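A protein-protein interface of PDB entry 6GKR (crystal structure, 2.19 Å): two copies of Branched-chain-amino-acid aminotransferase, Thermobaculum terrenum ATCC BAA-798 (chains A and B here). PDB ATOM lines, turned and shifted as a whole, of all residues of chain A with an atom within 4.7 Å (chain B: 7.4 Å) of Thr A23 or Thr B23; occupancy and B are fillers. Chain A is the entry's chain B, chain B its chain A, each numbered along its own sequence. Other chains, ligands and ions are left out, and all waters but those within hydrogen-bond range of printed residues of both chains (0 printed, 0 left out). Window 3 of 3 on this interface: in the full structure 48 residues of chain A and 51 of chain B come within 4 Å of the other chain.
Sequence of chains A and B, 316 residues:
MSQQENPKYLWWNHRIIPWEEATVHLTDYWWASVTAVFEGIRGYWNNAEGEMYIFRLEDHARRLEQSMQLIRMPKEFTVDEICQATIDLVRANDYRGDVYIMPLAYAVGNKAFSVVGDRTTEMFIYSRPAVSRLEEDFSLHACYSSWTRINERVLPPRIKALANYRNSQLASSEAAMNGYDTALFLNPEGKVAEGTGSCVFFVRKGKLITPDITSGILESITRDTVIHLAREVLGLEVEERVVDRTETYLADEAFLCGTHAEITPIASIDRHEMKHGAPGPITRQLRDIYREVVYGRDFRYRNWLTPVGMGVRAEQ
The backbone carbonyl oxygen (O) of Trp B19 is in hydrogen-bond range of a ring nitrogen (NE2) of His A25 (2.9 Å). The backbone NH of Leu B26 lies within hydrogen-bond range of the backbone carbonyl oxygen of Ala A22 (2.9 Å). The backbone carbonyl oxygen (O) of Val B24 sits at hydrogen-bond distance from the backbone NH (N) of Val A24, 2.8 Å away.
The side-chain hydroxyl of Thr B23 lies within hydrogen-bond range of the backbone carbonyl oxygen of Glu B20 (3.1 Å). OD2 of Asp B28 is in hydrogen-bond range of N of His B25 (2.9 Å).
His B25 touches Ala A22 (CD2 to O, 3.4 Å). CB of Thr A23 touches CG2 of Thr B23 (3.7 Å). Val B24 touches Thr A23 (O to CA, 3.2 Å). Thr B23 touches Val A24. Leu B26 touches Val A24 (N to CG2, 3.997 Å). CD2 of His A25 touches O of Ala B22, at 3.4 Å. His A25 touches Val B24 (C to CG2, 3.997 Å).
Of the printed residues of chain B, Thr A23 touches Thr B23 and Val B24. Of chain A, only Thr A23 (3.7 Å) and Val A24 (3.3 Å) come within 4 Å of Thr B23. Of the printed residues of chain A, His B25 touches Ala A22. Of the printed residues of chain A, Leu B26 touches Ala A22 and Val A24. Pro B18 touches none of the printed residues of chain A. The nearest residue of chain A that does not touch Thr B23 is His A25 (4.6 Å). The nearest printed residue of chain A that does not touch Leu B26 is Thr A23 (4.8 Å).
Of the 13 printed residues of chain B, 6 touch a printed residue of chain A. Printed residues of chain B that touch a printed residue of chain A: Trp B19, Ala B22, Thr B23, Val B24, His B25 and Leu B26. Hydrophobic or aromatic side chains of chain B that line the printed part of chain A: Trp B19, Ala B22, Val B24, His B25 and Leu B26. Of the 6 printed residues of chain A, 4 touch a printed residue of chain B. Hydrophobic or aromatic side chains of chain A within 4 Å of the printed part of chain B: Ala A22, Val A24 and His A25. Among the printed residues, 10 pairs touch across the chains. Among the printed residues, no Asp or Glu carboxylate lies within 4 Å of a Lys or Arg side-chain nitrogen of the other chain.
Ala A22 touches His B25, and with the chains exchanged His A25 touches Ala B22. Thr A23 touches its own counterpart, Thr B23. Val A24 touches its own counterpart, Val B24. His A25 touches Val B24, but with the chains exchanged Val A24 does not touch His B25 (4.01 Å). 6 positions are printed for both chains.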
ATOM      1  N   GLU A  20     -17.027  -4.887  12.843  1.00  0.00           N
ATOM      2  CA  GLU A  20     -17.700  -6.175  12.729  1.00  0.00           C
ATOM      3  C   GLU A  20     -16.705  -7.326  12.852  1.00  0.00           C
ATOM      4  O   GLU A  20     -17.103  -8.451  13.123  1.00  0.00           O
ATOM      5  CB  GLU A  20     -18.588  -6.296  11.481  1.00  0.00           C
ATOM      6  CG  GLU A  20     -20.036  -5.863  11.701  1.00  0.00           C
ATOM      7  CD  GLU A  20     -20.694  -6.104  13.057  1.00  0.00           C
ATOM      8  N   GLU A  21     -15.413  -7.040  12.694  1.00  0.00           N
ATOM      9  CA  GLU A  21     -14.437  -8.115  12.679  1.00  0.00           C
ATOM     10  C   GLU A  21     -13.971  -8.508  14.076  1.00  0.00           C
ATOM     11  O   GLU A  21     -13.245  -9.486  14.218  1.00  0.00           O
ATOM     12  CB  GLU A  21     -13.221  -7.696  11.862  1.00  0.00           C
ATOM     13  CG  GLU A  21     -13.403  -7.981  10.382  1.00  0.00           C
ATOM     14  CD  GLU A  21     -12.249  -7.436   9.552  1.00  0.00           C
ATOM     15  OE1 GLU A  21     -11.102  -7.356  10.085  1.00  0.00           O
ATOM     16  OE2 GLU A  21     -12.501  -7.042   8.399  1.00  0.00           O
ATOM     17  N   ALA A  22     -14.302  -7.707  15.092  1.00  0.00           N
ATOM     18  CA  ALA A  22     -13.785  -7.932  16.435  1.00  0.00           C
ATOM     19  C   ALA A  22     -14.781  -8.808  17.191  1.00  0.00           C
ATOM     20  O   ALA A  22     -15.371  -8.379  18.183  1.00  0.00           O
ATOM     21  CB  ALA A  22     -13.525  -6.595  17.118  1.00  0.00           C
ATOM     22  N   THR A  23     -15.003 -10.013  16.674  1.00  0.00           N
ATOM     23  CA  THR A  23     -15.904 -10.991  17.283  1.00  0.00           C
ATOM     24  C   THR A  23     -15.069 -11.946  18.133  1.00  0.00           C
ATOM     25  O   THR A  23     -13.910 -12.170  17.828  1.00  0.00           O
ATOM     26  CB  THR A  23     -16.726 -11.750  16.222  1.00  0.00           C
ATOM     27  OG1 THR A  23     -15.776 -12.237  15.266  1.00  0.00           O
ATOM     28  CG2 THR A  23     -17.769 -10.881  15.540  1.00  0.00           C
ATOM     29  N   VAL A  24     -15.637 -12.489  19.217  1.00  0.00           N
ATOM     30  CA  VAL A  24     -14.891 -13.277  20.178  1.00  0.00           C
ATOM     31  C   VAL A  24     -15.871 -14.288  20.742  1.00  0.00           C
ATOM     32  O   VAL A  24     -17.070 -14.230  20.438  1.00  0.00           O
ATOM     33  CB  VAL A  24     -14.297 -12.403  21.317  1.00  0.00           C
ATOM     34  CG1 VAL A  24     -13.344 -11.328  20.813  1.00  0.00           C
ATOM     35  CG2 VAL A  24     -15.367 -11.742  22.188  1.00  0.00           C
ATOM     36  N   HIS A  25     -15.381 -15.160  21.621  1.00  0.00           N
ATOM     37  CA  HIS A  25     -16.303 -16.083  22.256  1.00  0.00           C
ATOM     38  C   HIS A  25     -16.811 -15.483  23.563  1.00  0.00           C
ATOM     39  O   HIS A  25     -16.066 -14.773  24.241  1.00  0.00           O
ATOM     40  CB  HIS A  25     -15.643 -17.455  22.436  1.00  0.00           C
ATOM     41  CG  HIS A  25     -16.644 -18.508  22.774  1.00  0.00           C
ATOM     42  ND1 HIS A  25     -16.899 -18.873  24.088  1.00  0.00           N
ATOM     43  CD2 HIS A  25     -17.488 -19.229  22.000  1.00  0.00           C
ATOM     44  CE1 HIS A  25     -17.838 -19.798  24.111  1.00  0.00           C
ATOM     45  NE2 HIS A  25     -18.218 -20.033  22.838  1.00  0.00           N
ATOM     46  N   TRP B  12     -26.494 -21.013  28.089  1.00  0.00           N
ATOM     47  CA  TRP B  12     -26.510 -19.562  28.127  1.00  0.00           C
ATOM     48  C   TRP B  12     -27.958 -19.112  28.109  1.00  0.00           C
ATOM     49  O   TRP B  12     -28.703 -19.510  27.211  1.00  0.00           O
ATOM     50  CB  TRP B  12     -25.731 -18.994  26.935  1.00  0.00           C
ATOM     51  CG  TRP B  12     -25.480 -17.517  26.977  1.00  0.00           C
ATOM     52  CD1 TRP B  12     -25.450 -16.713  28.089  1.00  0.00           C
ATOM     53  CD2 TRP B  12     -25.116 -16.668  25.865  1.00  0.00           C
ATOM     54  NE1 TRP B  12     -25.120 -15.429  27.739  1.00  0.00           N
ATOM     55  CE2 TRP B  12     -24.890 -15.371  26.385  1.00  0.00           C
ATOM     56  CE3 TRP B  12     -24.950 -16.874  24.488  1.00  0.00           C
ATOM     57  CZ2 TRP B  12     -24.563 -14.273  25.569  1.00  0.00           C
ATOM     58  CZ3 TRP B  12     -24.609 -15.797  23.682  1.00  0.00           C
ATOM     59  CH2 TRP B  12     -24.440 -14.504  24.214  1.00  0.00           C
ATOM     60  N   ILE B  17     -26.486 -24.518  23.965  1.00  0.00           N
ATOM     61  CA  ILE B  17     -26.207 -24.074  22.614  1.00  0.00           C
ATOM     62  C   ILE B  17     -24.861 -24.645  22.185  1.00  0.00           C
ATOM     63  O   ILE B  17     -23.956 -24.823  23.003  1.00  0.00           O
ATOM     64  CB  ILE B  17     -26.236 -22.535  22.452  1.00  0.00           C
ATOM     65  CG1 ILE B  17     -25.232 -21.830  23.366  1.00  0.00           C
ATOM     66  CG2 ILE B  17     -27.633 -21.948  22.624  1.00  0.00           C
ATOM     67  CD1 ILE B  17     -25.009 -20.370  22.986  1.00  0.00           C
ATOM     68  N   PRO B  18     -24.675 -24.918  20.872  1.00  0.00           N
ATOM     69  CA  PRO B  18     -23.366 -25.309  20.352  1.00  0.00           C
ATOM     70  C   PRO B  18     -22.350 -24.213  20.680  1.00  0.00           C
ATOM     71  O   PRO B  18     -22.630 -23.013  20.586  1.00  0.00           O
ATOM     72  CB  PRO B  18     -23.606 -25.452  18.835  1.00  0.00           C
ATOM     73  CG  PRO B  18     -25.108 -25.692  18.711  1.00  0.00           C
ATOM     74  CD  PRO B  18     -25.726 -24.889  19.841  1.00  0.00           C
ATOM     75  N   TRP B  19     -21.151 -24.649  21.061  1.00  0.00           N
ATOM     76  CA  TRP B  19     -20.136 -23.725  21.514  1.00  0.00           C
ATOM     77  C   TRP B  19     -20.055 -22.497  20.595  1.00  0.00           C
ATOM     78  O   TRP B  19     -20.036 -21.364  21.073  1.00  0.00           O
ATOM     79  CB  TRP B  19     -18.811 -24.467  21.643  1.00  0.00           C
ATOM     80  CG  TRP B  19     -17.680 -23.575  22.072  1.00  0.00           C
ATOM     81  CD1 TRP B  19     -16.822 -22.862  21.273  1.00  0.00           C
ATOM     82  CD2 TRP B  19     -17.311 -23.278  23.430  1.00  0.00           C
ATOM     83  NE1 TRP B  19     -15.931 -22.158  22.046  1.00  0.00           N
ATOM     84  CE2 TRP B  19     -16.216 -22.383  23.369  1.00  0.00           C
ATOM     85  CE3 TRP B  19     -17.795 -23.685  24.676  1.00  0.00           C
ATOM     86  CZ2 TRP B  19     -15.601 -21.886  24.517  1.00  0.00           C
ATOM     87  CZ3 TRP B  19     -17.179 -23.206  25.810  1.00  0.00           C
ATOM     88  CH2 TRP B  19     -16.087 -22.328  25.728  1.00  0.00           C
ATOM     89  N   GLU B  20     -20.023 -22.713  19.274  1.00  0.00           N
ATOM     90  CA  GLU B  20     -19.647 -21.677  18.317  1.00  0.00           C
ATOM     91  C   GLU B  20     -20.784 -20.676  18.141  1.00  0.00           C
ATOM     92  O   GLU B  20     -20.584 -19.649  17.508  1.00  0.00           O
ATOM     93  CB  GLU B  20     -19.190 -22.271  16.974  1.00  0.00           C
ATOM     94  N   GLU B  21     -21.971 -20.925  18.703  1.00  0.00           N
ATOM     95  CA  GLU B  21     -23.040 -19.945  18.583  1.00  0.00           C
ATOM     96  C   GLU B  21     -22.931 -18.792  19.589  1.00  0.00           C
ATOM     97  O   GLU B  21     -23.628 -17.786  19.457  1.00  0.00           O
ATOM     98  CB  GLU B  21     -24.418 -20.570  18.762  1.00  0.00           C
ATOM     99  CG  GLU B  21     -24.979 -21.099  17.457  1.00  0.00           C
ATOM    100  CD  GLU B  21     -26.205 -21.967  17.659  1.00  0.00           C
ATOM    101  OE1 GLU B  21     -26.956 -21.738  18.653  1.00  0.00           O
ATOM    102  OE2 GLU B  21     -26.390 -22.877  16.840  1.00  0.00           O
ATOM    103  N   ALA B  22     -22.085 -18.954  20.616  1.00  0.00           N
ATOM    104  CA  ALA B  22     -21.953 -17.918  21.627  1.00  0.00           C
ATOM    105  C   ALA B  22     -20.821 -16.984  21.209  1.00  0.00           C
ATOM    106  O   ALA B  22     -19.877 -16.807  21.948  1.00  0.00           O
ATOM    107  CB  ALA B  22     -21.729 -18.549  22.987  1.00  0.00           C
ATOM    108  N   THR B  23     -20.893 -16.446  19.987  1.00  0.00           N
ATOM    109  CA  THR B  23     -19.971 -15.429  19.501  1.00  0.00           C
ATOM    110  C   THR B  23     -20.532 -14.053  19.852  1.00  0.00           C
ATOM    111  O   THR B  23     -21.751 -13.865  19.856  1.00  0.00           O
ATOM    112  CB  THR B  23     -19.769 -15.551  17.983  1.00  0.00           C
ATOM    113  OG1 THR B  23     -19.208 -16.838  17.786  1.00  0.00           O
ATOM    114  CG2 THR B  23     -18.798 -14.546  17.402  1.00  0.00           C
ATOM    115  N   VAL B  24     -19.640 -13.125  20.206  1.00  0.00           N
ATOM    116  CA  VAL B  24     -20.059 -11.847  20.749  1.00  0.00           C
ATOM    117  C   VAL B  24     -19.055 -10.810  20.276  1.00  0.00           C
ATOM    118  O   VAL B  24     -18.030 -11.145  19.684  1.00  0.00           O
ATOM    119  CB  VAL B  24     -20.130 -11.874  22.296  1.00  0.00           C
ATOM    120  CG1 VAL B  24     -21.119 -12.910  22.837  1.00  0.00           C
ATOM    121  CG2 VAL B  24     -18.771 -12.054  22.952  1.00  0.00           C
ATOM    122  N   HIS B  25     -19.314  -9.551  20.615  1.00  0.00           N
ATOM    123  CA  HIS B  25     -18.371  -8.522  20.233  1.00  0.00           C
ATOM    124  C   HIS B  25     -17.347  -8.334  21.361  1.00  0.00           C
ATOM    125  O   HIS B  25     -17.680  -8.491  22.544  1.00  0.00           O
ATOM    126  CB  HIS B  25     -19.120  -7.242  19.869  1.00  0.00           C
ATOM    127  CG  HIS B  25     -18.244  -6.269  19.169  1.00  0.00           C
ATOM    128  ND1 HIS B  25     -17.560  -5.275  19.840  1.00  0.00           N
ATOM    129  CD2 HIS B  25     -17.884  -6.166  17.877  1.00  0.00           C
ATOM    130  CE1 HIS B  25     -16.827  -4.586  18.986  1.00  0.00           C
ATOM    131  NE2 HIS B  25     -17.022  -5.100  17.769  1.00  0.00           N
ATOM    132  N   LEU B  26     -16.103  -8.000  20.992  1.00  0.00           N
ATOM    133  CA  LEU B  26     -15.057  -7.684  21.945  1.00  0.00           C
ATOM    134  C   LEU B  26     -15.550  -6.729  23.040  1.00  0.00           C
ATOM    135  O   LEU B  26     -15.170  -6.899  24.190  1.00  0.00           O
ATOM    136  CB  LEU B  26     -13.850  -7.069  21.218  1.00  0.00           C
ATOM    137  CG  LEU B  26     -12.704  -6.608  22.134  1.00  0.00           C
ATOM    138  CD1 LEU B  26     -12.152  -7.762  22.967  1.00  0.00           C
ATOM    139  CD2 LEU B  26     -11.574  -6.018  21.319  1.00  0.00           C
ATOM    140  N   ASP B  28     -18.532  -6.218  24.366  1.00  0.00           N
ATOM    141  CA  ASP B  28     -19.834  -6.520  24.953  1.00  0.00           C
ATOM    142  C   ASP B  28     -19.837  -6.605  26.480  1.00  0.00           C
ATOM    143  O   ASP B  28     -20.800  -6.172  27.082  1.00  0.00           O
ATOM    144  CB  ASP B  28     -20.444  -7.793  24.370  1.00  0.00           C
ATOM    145  CG  ASP B  28     -21.089  -7.588  23.011  1.00  0.00           C
ATOM    146  OD1 ASP B  28     -21.275  -6.418  22.631  1.00  0.00           O
ATOM    147  OD2 ASP B  28     -21.404  -8.599  22.341  1.00  0.00           O
ATOM    148  N   TYR B  29     -18.803  -7.183  27.114  1.00  0.00           N
ATOM    149  CA  TYR B  29     -18.971  -7.704  28.468  1.00  0.00           C
ATOM    150  C   TYR B  29     -18.049  -7.077  29.513  1.00  0.00           C
ATOM    151  O   TYR B  29     -18.063  -7.516  30.669  1.00  0.00           O
ATOM    152  CB  TYR B  29     -18.893  -9.235  28.484  1.00  0.00           C
ATOM    153  CG  TYR B  29     -20.088  -9.814  27.777  1.00  0.00           C
ATOM    154  CD1 TYR B  29     -21.368  -9.538  28.238  1.00  0.00           C
ATOM    155  CD2 TYR B  29     -19.959 -10.537  26.602  1.00  0.00           C
ATOM    156  CE1 TYR B  29     -22.490 -10.007  27.574  1.00  0.00           C
ATOM    157  CE2 TYR B  29     -21.075 -10.996  25.920  1.00  0.00           C
ATOM    158  CZ  TYR B  29     -22.342 -10.735  26.402  1.00  0.00           C
ATOM    159  OH  TYR B  29     -23.432 -11.172  25.713  1.00  0.00           O
